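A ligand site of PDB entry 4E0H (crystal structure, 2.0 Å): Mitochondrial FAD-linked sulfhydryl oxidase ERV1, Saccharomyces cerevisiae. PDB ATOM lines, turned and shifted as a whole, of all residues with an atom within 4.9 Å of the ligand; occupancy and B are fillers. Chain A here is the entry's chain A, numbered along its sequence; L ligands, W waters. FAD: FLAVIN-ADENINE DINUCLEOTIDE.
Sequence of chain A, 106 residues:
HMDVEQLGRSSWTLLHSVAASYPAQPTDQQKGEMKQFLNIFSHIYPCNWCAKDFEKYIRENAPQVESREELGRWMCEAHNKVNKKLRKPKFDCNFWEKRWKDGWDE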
ATOM      1  N   VAL A   4       7.956   1.189   0.330  1.00  0.00           N
ATOM      2  CA  VAL A   4       6.888   1.847   1.043  1.00  0.00           C
ATOM      3  C   VAL A   4       6.634   3.304   0.618  1.00  0.00           C
ATOM      4  O   VAL A   4       5.540   3.841   0.859  1.00  0.00           O
ATOM      5  CB  VAL A   4       6.980   1.708   2.596  1.00  0.00           C
ATOM      6  CG1 VAL A   4       7.214   0.253   3.007  1.00  0.00           C
ATOM      7  CG2 VAL A   4       8.060   2.577   3.149  1.00  0.00           C
ATOM      8  N   GLU A   5       7.650   3.949   0.021  1.00  0.00           N
ATOM      9  CA  GLU A   5       7.522   5.347  -0.392  1.00  0.00           C
ATOM     10  C   GLU A   5       6.638   5.498  -1.615  1.00  0.00           C
ATOM     11  O   GLU A   5       5.767   6.363  -1.634  1.00  0.00           O
ATOM     12  CB  GLU A   5       8.875   5.973  -0.708  1.00  0.00           C
ATOM     13  CG  GLU A   5       9.550   6.678   0.458  1.00  0.00           C
ATOM     14  CD  GLU A   5      10.928   7.255   0.063  1.00  0.00           C
ATOM     15  OE1 GLU A   5      11.152   7.595  -1.126  1.00  0.00           O
ATOM     16  OE2 GLU A   5      11.808   7.337   0.958  1.00  0.00           O
ATOM     17  N   GLY A   8       3.236   4.333  -0.855  1.00  0.00           N
ATOM     18  CA  GLY A   8       2.581   5.373  -0.007  1.00  0.00           C
ATOM     19  C   GLY A   8       2.107   6.555  -0.814  1.00  0.00           C
ATOM     20  O   GLY A   8       0.946   6.919  -0.726  1.00  0.00           O
ATOM     21  N   ARG A   9       2.967   7.177  -1.627  1.00  0.00           N
ATOM     22  CA  ARG A   9       2.529   8.278  -2.479  1.00  0.00           C
ATOM     23  C   ARG A   9       1.394   7.857  -3.393  1.00  0.00           C
ATOM     24  O   ARG A   9       0.440   8.618  -3.549  1.00  0.00           O
ATOM     25  CB  ARG A   9       3.604   8.751  -3.433  1.00  0.00           C
ATOM     26  CG  ARG A   9       4.585   9.578  -2.878  1.00  0.00           C
ATOM     27  CD  ARG A   9       5.524  10.121  -3.952  1.00  0.00           C
ATOM     28  NE  ARG A   9       6.444   9.057  -4.314  1.00  0.00           N
ATOM     29  CZ  ARG A   9       7.593   8.766  -3.678  1.00  0.00           C
ATOM     30  NH1 ARG A   9       8.015   9.446  -2.623  1.00  0.00           N
ATOM     31  NH2 ARG A   9       8.324   7.752  -4.113  1.00  0.00           N
ATOM     32  N   SER A  11      -0.801   5.528  -2.955  1.00  0.00           N
ATOM     33  CA  SER A  11      -2.035   5.212  -2.222  1.00  0.00           C
ATOM     34  C   SER A  11      -2.696   6.483  -1.680  1.00  0.00           C
ATOM     35  O   SER A  11      -3.900   6.595  -1.744  1.00  0.00           O
ATOM     36  CB  SER A  11      -1.783   4.154  -1.116  1.00  0.00           C
ATOM     37  OG  SER A  11      -1.266   2.955  -1.665  1.00  0.00           O
ATOM     38  N   TRP A  12      -1.918   7.457  -1.218  1.00  0.00           N
ATOM     39  CA  TRP A  12      -2.519   8.760  -0.847  1.00  0.00           C
ATOM     40  C   TRP A  12      -3.128   9.465  -2.070  1.00  0.00           C
ATOM     41  O   TRP A  12      -4.182  10.065  -1.953  1.00  0.00           O
ATOM     42  CB  TRP A  12      -1.496   9.705  -0.196  1.00  0.00           C
ATOM     43  CG  TRP A  12      -1.041   9.225   1.197  1.00  0.00           C
ATOM     44  CD1 TRP A  12       0.200   8.910   1.560  1.00  0.00           C
ATOM     45  CD2 TRP A  12      -1.856   9.048   2.360  1.00  0.00           C
ATOM     46  NE1 TRP A  12       0.238   8.518   2.890  1.00  0.00           N
ATOM     47  CE2 TRP A  12      -1.019   8.646   3.401  1.00  0.00           C
ATOM     48  CE3 TRP A  12      -3.205   9.211   2.620  1.00  0.00           C
ATOM     49  CZ2 TRP A  12      -1.478   8.368   4.664  1.00  0.00           C
ATOM     50  CZ3 TRP A  12      -3.669   8.941   3.906  1.00  0.00           C
ATOM     51  CH2 TRP A  12      -2.806   8.487   4.890  1.00  0.00           C
ATOM     52  N   LEU A  15      -6.504   7.794  -2.420  1.00  0.00           N
ATOM     53  CA  LEU A  15      -7.454   8.175  -1.353  1.00  0.00           C
ATOM     54  C   LEU A  15      -8.003   9.588  -1.412  1.00  0.00           C
ATOM     55  O   LEU A  15      -9.216   9.797  -1.280  1.00  0.00           O
ATOM     56  CB  LEU A  15      -6.793   7.986   0.032  1.00  0.00           C
ATOM     57  CG  LEU A  15      -6.471   6.525   0.387  1.00  0.00           C
ATOM     58  CD1 LEU A  15      -5.638   6.378   1.662  1.00  0.00           C
ATOM     59  CD2 LEU A  15      -7.821   5.850   0.600  1.00  0.00           C
ATOM     60  N   HIS A  16      -7.105  10.563  -1.565  1.00  0.00           N
ATOM     61  CA  HIS A  16      -7.472  11.999  -1.712  1.00  0.00           C
ATOM     62  C   HIS A  16      -8.267  12.258  -3.010  1.00  0.00           C
ATOM     63  O   HIS A  16      -9.157  13.077  -2.993  1.00  0.00           O
ATOM     64  CB  HIS A  16      -6.243  12.912  -1.696  1.00  0.00           C
ATOM     65  CG  HIS A  16      -5.555  12.955  -0.346  1.00  0.00           C
ATOM     66  ND1 HIS A  16      -6.210  13.342   0.797  1.00  0.00           N
ATOM     67  CD2 HIS A  16      -4.287  12.665   0.024  1.00  0.00           C
ATOM     68  CE1 HIS A  16      -5.385  13.262   1.826  1.00  0.00           C
ATOM     69  NE2 HIS A  16      -4.211  12.858   1.391  1.00  0.00           N
ATOM     70  N   PHE A  41      -9.518  -1.185   3.093  1.00  0.00           N
ATOM     71  CA  PHE A  41      -8.195  -0.640   2.725  1.00  0.00           C
ATOM     72  C   PHE A  41      -7.217  -0.816   3.881  1.00  0.00           C
ATOM     73  O   PHE A  41      -6.070  -1.251   3.712  1.00  0.00           O
ATOM     74  CB  PHE A  41      -8.339   0.849   2.359  1.00  0.00           C
ATOM     75  CG  PHE A  41      -7.023   1.492   1.989  1.00  0.00           C
ATOM     76  CD1 PHE A  41      -6.568   1.475   0.685  1.00  0.00           C
ATOM     77  CD2 PHE A  41      -6.246   2.118   2.941  1.00  0.00           C
ATOM     78  CE1 PHE A  41      -5.327   2.065   0.355  1.00  0.00           C
ATOM     79  CE2 PHE A  41      -5.005   2.708   2.610  1.00  0.00           C
ATOM     80  CZ  PHE A  41      -4.562   2.671   1.336  1.00  0.00           C
ATOM     81  N   TYR A  45      -3.848  -3.010   3.223  1.00  0.00           N
ATOM     82  CA  TYR A  45      -2.748  -2.160   2.778  1.00  0.00           C
ATOM     83  C   TYR A  45      -1.424  -2.896   2.954  1.00  0.00           C
ATOM     84  O   TYR A  45      -1.071  -3.322   4.075  1.00  0.00           O
ATOM     85  CB  TYR A  45      -2.710  -0.849   3.543  1.00  0.00           C
ATOM     86  CG  TYR A  45      -1.702   0.097   2.969  1.00  0.00           C
ATOM     87  CD1 TYR A  45      -1.861   0.637   1.687  1.00  0.00           C
ATOM     88  CD2 TYR A  45      -0.570   0.472   3.696  1.00  0.00           C
ATOM     89  CE1 TYR A  45      -0.917   1.535   1.156  1.00  0.00           C
ATOM     90  CE2 TYR A  45       0.375   1.348   3.168  1.00  0.00           C
ATOM     91  CZ  TYR A  45       0.179   1.877   1.924  1.00  0.00           C
ATOM     92  OH  TYR A  45       1.107   2.752   1.437  1.00  0.00           O
ATOM     93  N   TRP A  49       2.768  -2.662   9.296  1.00  0.00           N
ATOM     94  CA  TRP A  49       2.675  -1.715  10.420  1.00  0.00           C
ATOM     95  C   TRP A  49       1.905  -0.425  10.076  1.00  0.00           C
ATOM     96  O   TRP A  49       1.116   0.059  10.878  1.00  0.00           O
ATOM     97  CB  TRP A  49       4.068  -1.383  10.971  1.00  0.00           C
ATOM     98  CG  TRP A  49       5.014  -0.628  10.026  1.00  0.00           C
ATOM     99  CD1 TRP A  49       5.166   0.728   9.931  1.00  0.00           C
ATOM    100  CD2 TRP A  49       5.977  -1.205   9.114  1.00  0.00           C
ATOM    101  NE1 TRP A  49       6.153   1.040   8.994  1.00  0.00           N
ATOM    102  CE2 TRP A  49       6.658  -0.123   8.487  1.00  0.00           C
ATOM    103  CE3 TRP A  49       6.320  -2.533   8.775  1.00  0.00           C
ATOM    104  CZ2 TRP A  49       7.663  -0.312   7.521  1.00  0.00           C
ATOM    105  CZ3 TRP A  49       7.313  -2.727   7.803  1.00  0.00           C
ATOM    106  CH2 TRP A  49       7.976  -1.622   7.192  1.00  0.00           C
ATOM    107  N   CYS A  50       2.174   0.111   8.872  1.00  0.00           N
ATOM    108  CA  CYS A  50       1.346   1.119   8.214  1.00  0.00           C
ATOM    109  C   CYS A  50      -0.154   0.765   8.364  1.00  0.00           C
ATOM    110  O   CYS A  50      -0.947   1.546   8.914  1.00  0.00           O
ATOM    111  CB  CYS A  50       1.687   1.190   6.703  1.00  0.00           C
ATOM    112  SG  CYS A  50       3.417   1.624   6.122  1.00  0.00           S
ATOM    113  N   PHE A  54      -3.299   2.640  10.789  1.00  0.00           N
ATOM    114  CA  PHE A  54      -4.310   3.361  10.063  1.00  0.00           C
ATOM    115  C   PHE A  54      -5.626   2.719  10.411  1.00  0.00           C
ATOM    116  O   PHE A  54      -6.619   3.427  10.596  1.00  0.00           O
ATOM    117  CB  PHE A  54      -4.017   3.351   8.540  1.00  0.00           C
ATOM    118  CG  PHE A  54      -5.036   4.131   7.712  1.00  0.00           C
ATOM    119  CD1 PHE A  54      -5.209   5.491   7.901  1.00  0.00           C
ATOM    120  CD2 PHE A  54      -5.796   3.492   6.755  1.00  0.00           C
ATOM    121  CE1 PHE A  54      -6.161   6.213   7.119  1.00  0.00           C
ATOM    122  CE2 PHE A  54      -6.722   4.206   5.964  1.00  0.00           C
ATOM    123  CZ  PHE A  54      -6.911   5.556   6.161  1.00  0.00           C
ATOM    124  N   MET A  75      -9.604  12.839   5.560  1.00  0.00           N
ATOM    125  CA  MET A  75      -8.440  12.276   4.870  1.00  0.00           C
ATOM    126  C   MET A  75      -7.188  13.121   5.084  1.00  0.00           C
ATOM    127  O   MET A  75      -6.092  12.591   5.288  1.00  0.00           O
ATOM    128  CB  MET A  75      -8.751  12.251   3.344  1.00  0.00           C
ATOM    129  CG  MET A  75      -8.058  11.090   2.587  1.00  0.00           C
ATOM    130  SD  MET A  75      -8.522   9.433   3.202  1.00  0.00           S
ATOM    131  CE  MET A  75     -10.166   9.360   2.539  1.00  0.00           C
ATOM    132  N   CYS A  76      -7.323  14.429   4.960  1.00  0.00           N
ATOM    133  CA  CYS A  76      -6.211  15.324   5.201  1.00  0.00           C
ATOM    134  C   CYS A  76      -5.639  15.108   6.626  1.00  0.00           C
ATOM    135  O   CYS A  76      -4.416  15.031   6.819  1.00  0.00           O
ATOM    136  CB  CYS A  76      -6.621  16.766   4.951  1.00  0.00           C
ATOM    137  SG  CYS A  76      -5.268  17.949   5.148  1.00  0.00           S
ATOM    138  N   HIS A  79      -3.874  11.639   6.911  1.00  0.00           N
ATOM    139  CA  HIS A  79      -2.546  11.782   6.297  1.00  0.00           C
ATOM    140  C   HIS A  79      -1.587  12.588   7.191  1.00  0.00           C
ATOM    141  O   HIS A  79      -0.418  12.237   7.316  1.00  0.00           O
ATOM    142  CB  HIS A  79      -2.719  12.445   4.925  1.00  0.00           C
ATOM    143  CG  HIS A  79      -1.513  12.336   4.028  1.00  0.00           C
ATOM    144  ND1 HIS A  79      -1.582  12.543   2.674  1.00  0.00           N
ATOM    145  CD2 HIS A  79      -0.227  12.072   4.311  1.00  0.00           C
ATOM    146  CE1 HIS A  79      -0.377  12.445   2.146  1.00  0.00           C
ATOM    147  NE2 HIS A  79       0.472  12.144   3.123  1.00  0.00           N
ATOM    148  N   ASN A  80      -2.065  13.655   7.821  1.00  0.00           N
ATOM    149  CA  ASN A  80      -1.246  14.464   8.738  1.00  0.00           C
ATOM    150  C   ASN A  80      -0.819  13.719   9.976  1.00  0.00           C
ATOM    151  O   ASN A  80       0.247  14.000  10.536  1.00  0.00           O
ATOM    152  CB  ASN A  80      -1.965  15.735   9.162  1.00  0.00           C
ATOM    153  CG  ASN A  80      -1.635  16.885   8.253  1.00  0.00           C
ATOM    154  OD1 ASN A  80      -0.596  16.900   7.590  1.00  0.00           O
ATOM    155  ND2 ASN A  80      -2.489  17.861   8.242  1.00  0.00           N
ATOM    156  N   VAL A  82       0.026  10.598   9.926  1.00  0.00           N
ATOM    157  CA  VAL A  82       1.150   9.866   9.419  1.00  0.00           C
ATOM    158  C   VAL A  82       2.366  10.777   9.180  1.00  0.00           C
ATOM    159  O   VAL A  82       3.496  10.414   9.540  1.00  0.00           O
ATOM    160  CB  VAL A  82       0.745   9.083   8.155  1.00  0.00           C
ATOM    161  CG1 VAL A  82       1.932   8.436   7.545  1.00  0.00           C
ATOM    162  CG2 VAL A  82      -0.311   8.103   8.493  1.00  0.00           C
ATOM    163  N   ASN A  83       2.164  11.966   8.578  1.00  0.00           N
ATOM    164  CA  ASN A  83       3.219  12.975   8.477  1.00  0.00           C
ATOM    165  C   ASN A  83       3.864  13.278   9.858  1.00  0.00           C
ATOM    166  O   ASN A  83       5.068  13.399   9.984  1.00  0.00           O
ATOM    167  CB  ASN A  83       2.653  14.308   7.935  1.00  0.00           C
ATOM    168  CG  ASN A  83       2.255  14.211   6.455  1.00  0.00           C
ATOM    169  OD1 ASN A  83       2.760  13.357   5.717  1.00  0.00           O
ATOM    170  ND2 ASN A  83       1.386  15.127   6.013  1.00  0.00           N
ATOM    171  N   LYS A  85       4.029  11.327  12.715  1.00  0.00           N
ATOM    172  CA  LYS A  85       4.755  10.077  12.939  1.00  0.00           C
ATOM    173  C   LYS A  85       6.090  10.008  12.148  1.00  0.00           C
ATOM    174  O   LYS A  85       7.084   9.529  12.658  1.00  0.00           O
ATOM    175  CB  LYS A  85       3.816   8.896  12.596  1.00  0.00           C
ATOM    176  CG  LYS A  85       4.350   7.467  12.784  1.00  0.00           C
ATOM    177  CD  LYS A  85       3.409   6.383  12.142  1.00  0.00           C
ATOM    178  CE  LYS A  85       3.897   4.953  12.490  1.00  0.00           C
ATOM    179  NZ  LYS A  85       3.506   3.806  11.549  1.00  0.00           N
ATOM    180  N   LEU A  86       6.130  10.537  10.929  1.00  0.00           N
ATOM    181  CA  LEU A  86       7.345  10.427  10.127  1.00  0.00           C
ATOM    182  C   LEU A  86       8.200  11.675  10.145  1.00  0.00           C
ATOM    183  O   LEU A  86       9.127  11.775   9.352  1.00  0.00           O
ATOM    184  CB  LEU A  86       7.017  10.083   8.656  1.00  0.00           C
ATOM    185  CG  LEU A  86       6.177   8.837   8.391  1.00  0.00           C
ATOM    186  CD1 LEU A  86       6.000   8.633   6.881  1.00  0.00           C
ATOM    187  CD2 LEU A  86       6.775   7.626   9.086  1.00  0.00           C
ATOM    188  N   LYS A  88       7.518  14.651   8.986  1.00  0.00           N
ATOM    189  CA  LYS A  88       7.328  15.474   7.815  1.00  0.00           C
ATOM    190  C   LYS A  88       6.489  16.657   8.246  1.00  0.00           C
ATOM    191  O   LYS A  88       5.844  16.610   9.321  1.00  0.00           O
ATOM    192  CB  LYS A  88       6.578  14.689   6.735  1.00  0.00           C
ATOM    193  CG  LYS A  88       7.382  13.559   6.059  1.00  0.00           C
ATOM    194  CD  LYS A  88       6.429  12.589   5.296  1.00  0.00           C
ATOM    195  CE  LYS A  88       7.173  11.613   4.371  1.00  0.00           C
ATOM    196  NZ  LYS A  88       7.815  12.397   3.272  1.00  0.00           N
ATOM    197  N   PHE A  91       0.599  19.407   6.516  1.00  0.00           N
ATOM    198  CA  PHE A  91      -0.137  19.961   5.346  1.00  0.00           C
ATOM    199  C   PHE A  91      -1.304  20.797   5.832  1.00  0.00           C
ATOM    200  O   PHE A  91      -2.042  20.395   6.715  1.00  0.00           O
ATOM    201  CB  PHE A  91      -0.656  18.788   4.471  1.00  0.00           C
ATOM    202  CG  PHE A  91      -1.289  19.215   3.137  1.00  0.00           C
ATOM    203  CD1 PHE A  91      -2.642  19.487   3.055  1.00  0.00           C
ATOM    204  CD2 PHE A  91      -0.504  19.284   1.991  1.00  0.00           C
ATOM    205  CE1 PHE A  91      -3.242  19.845   1.837  1.00  0.00           C
ATOM    206  CE2 PHE A  91      -1.093  19.670   0.776  1.00  0.00           C
ATOM    207  CZ  PHE A  91      -2.435  19.948   0.699  1.00  0.00           C
ATOM    208  N   TRP A  96      -6.597  21.571   1.046  1.00  0.00           N
ATOM    209  CA  TRP A  96      -6.883  20.233   0.582  1.00  0.00           C
ATOM    210  C   TRP A  96      -7.660  20.278  -0.745  1.00  0.00           C
ATOM    211  O   TRP A  96      -7.318  19.563  -1.656  1.00  0.00           O
ATOM    212  CB  TRP A  96      -7.725  19.459   1.641  1.00  0.00           C
ATOM    213  CG  TRP A  96      -8.011  18.111   1.167  1.00  0.00           C
ATOM    214  CD1 TRP A  96      -7.193  17.021   1.253  1.00  0.00           C
ATOM    215  CD2 TRP A  96      -9.168  17.689   0.436  1.00  0.00           C
ATOM    216  NE1 TRP A  96      -7.811  15.911   0.682  1.00  0.00           N
ATOM    217  CE2 TRP A  96      -8.995  16.315   0.130  1.00  0.00           C
ATOM    218  CE3 TRP A  96     -10.348  18.334   0.042  1.00  0.00           C
ATOM    219  CZ2 TRP A  96      -9.952  15.579  -0.602  1.00  0.00           C
ATOM    220  CZ3 TRP A  96     -11.313  17.594  -0.686  1.00  0.00           C
ATOM    221  CH2 TRP A  96     -11.096  16.232  -0.991  1.00  0.00           C
ATOM    222  N   ARG A  99      -5.618  21.540  -3.758  1.00  0.00           N
ATOM    223  CA  ARG A  99      -4.620  20.554  -4.175  1.00  0.00           C
ATOM    224  C   ARG A  99      -5.258  19.384  -4.860  1.00  0.00           C
ATOM    225  O   ARG A  99      -4.744  18.948  -5.862  1.00  0.00           O
ATOM    226  CB  ARG A  99      -3.832  20.012  -2.962  1.00  0.00           C
ATOM    227  CG  ARG A  99      -3.037  18.751  -3.244  1.00  0.00           C
ATOM    228  CD  ARG A  99      -1.799  19.051  -4.041  1.00  0.00           C
ATOM    229  NE  ARG A  99      -1.006  17.854  -4.277  1.00  0.00           N
ATOM    230  CZ  ARG A  99      -1.268  16.933  -5.207  1.00  0.00           C
ATOM    231  NH1 ARG A  99      -2.337  17.074  -6.027  1.00  0.00           N
ATOM    232  NH2 ARG A  99      -0.434  15.888  -5.341  1.00  0.00           N
ATOM    233  N   TRP A 100      -6.312  18.834  -4.306  1.00  0.00           N
ATOM    234  CA  TRP A 100      -6.802  17.524  -4.746  1.00  0.00           C
ATOM    235  C   TRP A 100      -8.054  17.602  -5.580  1.00  0.00           C
ATOM    236  O   TRP A 100      -8.264  16.797  -6.473  1.00  0.00           O
ATOM    237  CB  TRP A 100      -7.032  16.589  -3.540  1.00  0.00           C
ATOM    238  CG  TRP A 100      -5.756  16.143  -2.975  1.00  0.00           C
ATOM    239  CD1 TRP A 100      -5.172  16.539  -1.790  1.00  0.00           C
ATOM    240  CD2 TRP A 100      -4.808  15.280  -3.609  1.00  0.00           C
ATOM    241  NE1 TRP A 100      -3.941  15.925  -1.639  1.00  0.00           N
ATOM    242  CE2 TRP A 100      -3.701  15.157  -2.741  1.00  0.00           C
ATOM    243  CE3 TRP A 100      -4.813  14.558  -4.803  1.00  0.00           C
ATOM    244  CZ2 TRP A 100      -2.600  14.355  -3.043  1.00  0.00           C
ATOM    245  CZ3 TRP A 100      -3.724  13.750  -5.110  1.00  0.00           C
ATOM    246  CH2 TRP A 100      -2.632  13.663  -4.231  1.00  0.00           C
HETATM  247  PA  FAD L   1       3.258  11.632   0.712  1.00  0.00           P
HETATM  248  O1A FAD L   1       2.905  10.250   0.216  1.00  0.00           O
HETATM  249  O2A FAD L   1       3.186  11.749   2.227  1.00  0.00           O
HETATM  250  O5B FAD L   1       2.300  12.696   0.032  1.00  0.00           O
HETATM  251  C5B FAD L   1       1.925  12.764  -1.341  1.00  0.00           C
HETATM  252  C4B FAD L   1       1.488  14.205  -1.624  1.00  0.00           C
HETATM  253  O4B FAD L   1       0.311  14.452  -0.891  1.00  0.00           O
HETATM  254  C3B FAD L   1       2.408  15.272  -1.070  1.00  0.00           C
HETATM  255  O3B FAD L   1       3.438  15.480  -1.987  1.00  0.00           O
HETATM  256  C2B FAD L   1       1.530  16.492  -0.824  1.00  0.00           C
HETATM  257  O2B FAD L   1       1.268  17.242  -1.999  1.00  0.00           O
HETATM  258  C1B FAD L   1       0.198  15.821  -0.520  1.00  0.00           C
HETATM  259  N9A FAD L   1      -0.053  15.822   0.954  1.00  0.00           N
HETATM  260  C8A FAD L   1       0.868  15.716   1.970  1.00  0.00           C
HETATM  261  N7A FAD L   1       0.174  15.693   3.149  1.00  0.00           N
HETATM  262  C5A FAD L   1      -1.152  15.797   2.906  1.00  0.00           C
HETATM  263  C6A FAD L   1      -2.286  15.846   3.729  1.00  0.00           C
HETATM  264  N6A FAD L   1      -2.283  15.841   5.101  1.00  0.00           N
HETATM  265  N1A FAD L   1      -3.468  15.949   3.091  1.00  0.00           N
HETATM  266  C2A FAD L   1      -3.593  16.002   1.728  1.00  0.00           C
HETATM  267  N3A FAD L   1      -2.477  15.963   0.955  1.00  0.00           N
HETATM  268  C4A FAD L   1      -1.285  15.857   1.535  1.00  0.00           C
HETATM  269  N1  FAD L   1       5.318   5.264   5.624  1.00  0.00           N
HETATM  270  C2  FAD L   1       6.103   5.011   6.729  1.00  0.00           C
HETATM  271  O2  FAD L   1       7.327   5.123   6.630  1.00  0.00           O
HETATM  272  N3  FAD L   1       5.526   4.674   7.940  1.00  0.00           N
HETATM  273  C4  FAD L   1       4.151   4.547   8.069  1.00  0.00           C
HETATM  274  O4  FAD L   1       3.622   4.233   9.148  1.00  0.00           O
HETATM  275  C4X FAD L   1       3.356   4.784   6.949  1.00  0.00           C
HETATM  276  N5  FAD L   1       1.990   4.664   7.052  1.00  0.00           N
HETATM  277  C5X FAD L   1       1.218   4.858   5.907  1.00  0.00           C
HETATM  278  C6  FAD L   1      -0.155   4.723   6.005  1.00  0.00           C
HETATM  279  C7  FAD L   1      -0.955   4.913   4.872  1.00  0.00           C
HETATM  280  C7M FAD L   1      -2.439   4.787   4.958  1.00  0.00           C
HETATM  281  C8  FAD L   1      -0.377   5.297   3.642  1.00  0.00           C
HETATM  282  C8M FAD L   1      -1.253   5.496   2.441  1.00  0.00           C
HETATM  283  C9  FAD L   1       1.004   5.447   3.551  1.00  0.00           C
HETATM  284  C9A FAD L   1       1.809   5.238   4.673  1.00  0.00           C
HETATM  285  N10 FAD L   1       3.199   5.412   4.629  1.00  0.00           N
HETATM  286  C10 FAD L   1       3.956   5.133   5.749  1.00  0.00           C
HETATM  287  C1' FAD L   1       3.946   6.248   3.599  1.00  0.00           C
HETATM  288  C2' FAD L   1       4.049   7.765   3.794  1.00  0.00           C
HETATM  289  O2' FAD L   1       2.826   8.234   4.228  1.00  0.00           O
HETATM  290  C3' FAD L   1       4.403   8.488   2.494  1.00  0.00           C
HETATM  291  O3' FAD L   1       3.522   8.189   1.425  1.00  0.00           O
HETATM  292  C4' FAD L   1       5.788   8.171   1.928  1.00  0.00           C
HETATM  293  O4' FAD L   1       6.760   8.354   2.923  1.00  0.00           O
HETATM  294  C5' FAD L   1       6.057   9.069   0.733  1.00  0.00           C
HETATM  295  O5' FAD L   1       6.147  10.404   1.201  1.00  0.00           O
HETATM  296  P   FAD L   1       6.111  11.669   0.238  1.00  0.00           P
HETATM  297  O1P FAD L   1       6.929  12.745   0.875  1.00  0.00           O
HETATM  298  O2P FAD L   1       6.570  11.307  -1.124  1.00  0.00           O
HETATM  299  O3P FAD L   1       4.639  12.198   0.132  1.00  0.00           O
HETATM  300  O   HOH W   1       3.430  10.821   4.634  1.00  0.00           O
HETATM  301  O   HOH W   2       2.471  16.263  -4.788  1.00  0.00           O
HETATM  302  O   HOH W   3       3.668   3.086   2.462  1.00  0.00           O
HETATM  303  O   HOH W   4       3.788  14.425   3.187  1.00  0.00           O
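Water W1 bridges an oxygen (O2A) of the ligand (2.6 Å) and the side-chain amide oxygen (OD1) of Asn 83 (2.8 Å).
Water W4 lies within hydrogen-bond range of an oxygen (O2A) of the ligand and the side-chain amide oxygen of Asn 83.
Water W2 lies within hydrogen-bond range of the guanidinium group (NH2) of Arg 99 (3.0 Å) and an oxygen (O3B) of the ligand (3.1 Å).
Water W3 bridges the backbone carbonyl oxygen (O) of Val 4 (2.6 Å) and the side-chain hydroxyl (OH) of Tyr 45 (2.8 Å).
The side-chain sulfur (SG) of Cys 50 sits close to a nitrogen (N5) of the ligand, at 3.5 Å.
O of Val 4 touches C1' of the ligand, at 3.98 Å.
Glu 5 touches the ligand (O to C5', 3.6 Å).
Gly 8 touches the ligand (C to O3', 3.1 Å).
Ser 11 touches the ligand (CB to C8M, 3.8 Å).
His 16 touches the ligand (NE2 to C2A, 3.2 Å).
Tyr 45 touches the ligand.
Trp 49 touches the ligand (NE1 to N3, 3.8 Å).
Phe 54 touches the ligand (CG to C7M, 3.8 Å).
Val 82 touches the ligand (CG1 to O2', 3.4 Å).
Leu 86 touches the ligand.
CB of Phe 91 touches C5A of the ligand, at 3.4 Å.
Trp 96 touches the ligand (CD1 to C2A, 3.8 Å).
Of the 26 residues printed, 23 come within 4 Å of the ligand.
The nearest printed residue that does not touch the ligand is Phe 41 (4.1 Å).
ND1 of His 16 is in hydrogen-bond range of NE1 of Trp 96, 3.0 Å away.
The backbone NH (N) of Lys 88 lies within hydrogen-bond range of the backbone carbonyl oxygen (O) of Asn 83 (2.9 Å).
The guanidinium group of Arg 9 is in salt-bridge range of the side-chain carboxylate of Glu 5, 3.9 Å away.
NE2 of His 16 is in hydrogen-bond range of ND1 of His 79 (2.9 Å).
OD1 of Asn 80 is in hydrogen-bond range of N of Phe 91, 3.0 Å away.
The side-chain amide oxygen (OD1) of Asn 80 is in hydrogen-bond range of the side-chain amide nitrogen (ND2) of Asn 83 (3.1 Å).
NE1 of Trp 12 lies within hydrogen-bond range of O2' of the ligand, 2.9 Å away.
A ring nitrogen (NE2) of His 79 sits at hydrogen-bond distance from an oxygen (O2A) of the ligand (2.9 Å).
The guanidinium group (NH1) of Arg 9 is in salt-bridge range of an oxygen (O2P) of the ligand (2.8 Å).
N of Arg 9 is in hydrogen-bond range of O3' of the ligand, 3.3 Å away.
N6A of the ligand lies within hydrogen-bond range of OD1 of Asn 80 (3.2 Å).
The backbone carbonyl oxygen of Cys 76 is in hydrogen-bond range of a nitrogen (N6A) of the ligand (2.9 Å).
An oxygen (O1P) of the ligand lies within salt-bridge range of the side-chain amino group of Lys 88, 2.6 Å away.
NE of Arg 99 sits at hydrogen-bond distance from O2B of the ligand, at 3.3 Å.
NE1 of Trp 100 sits at hydrogen-bond distance from N3A of the ligand, 3.0 Å away.
A nitrogen (N7A) of the ligand lies within hydrogen-bond range of the side-chain amide nitrogen of Asn 83.
The side-chain amino group (NZ) of Lys 85 sits at hydrogen-bond distance from an oxygen (O4) of the ligand (2.4 Å).
A nitrogen (N6A) of the ligand sits at hydrogen-bond distance from the side-chain sulfur (SG) of Cys 76 (3.7 Å).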
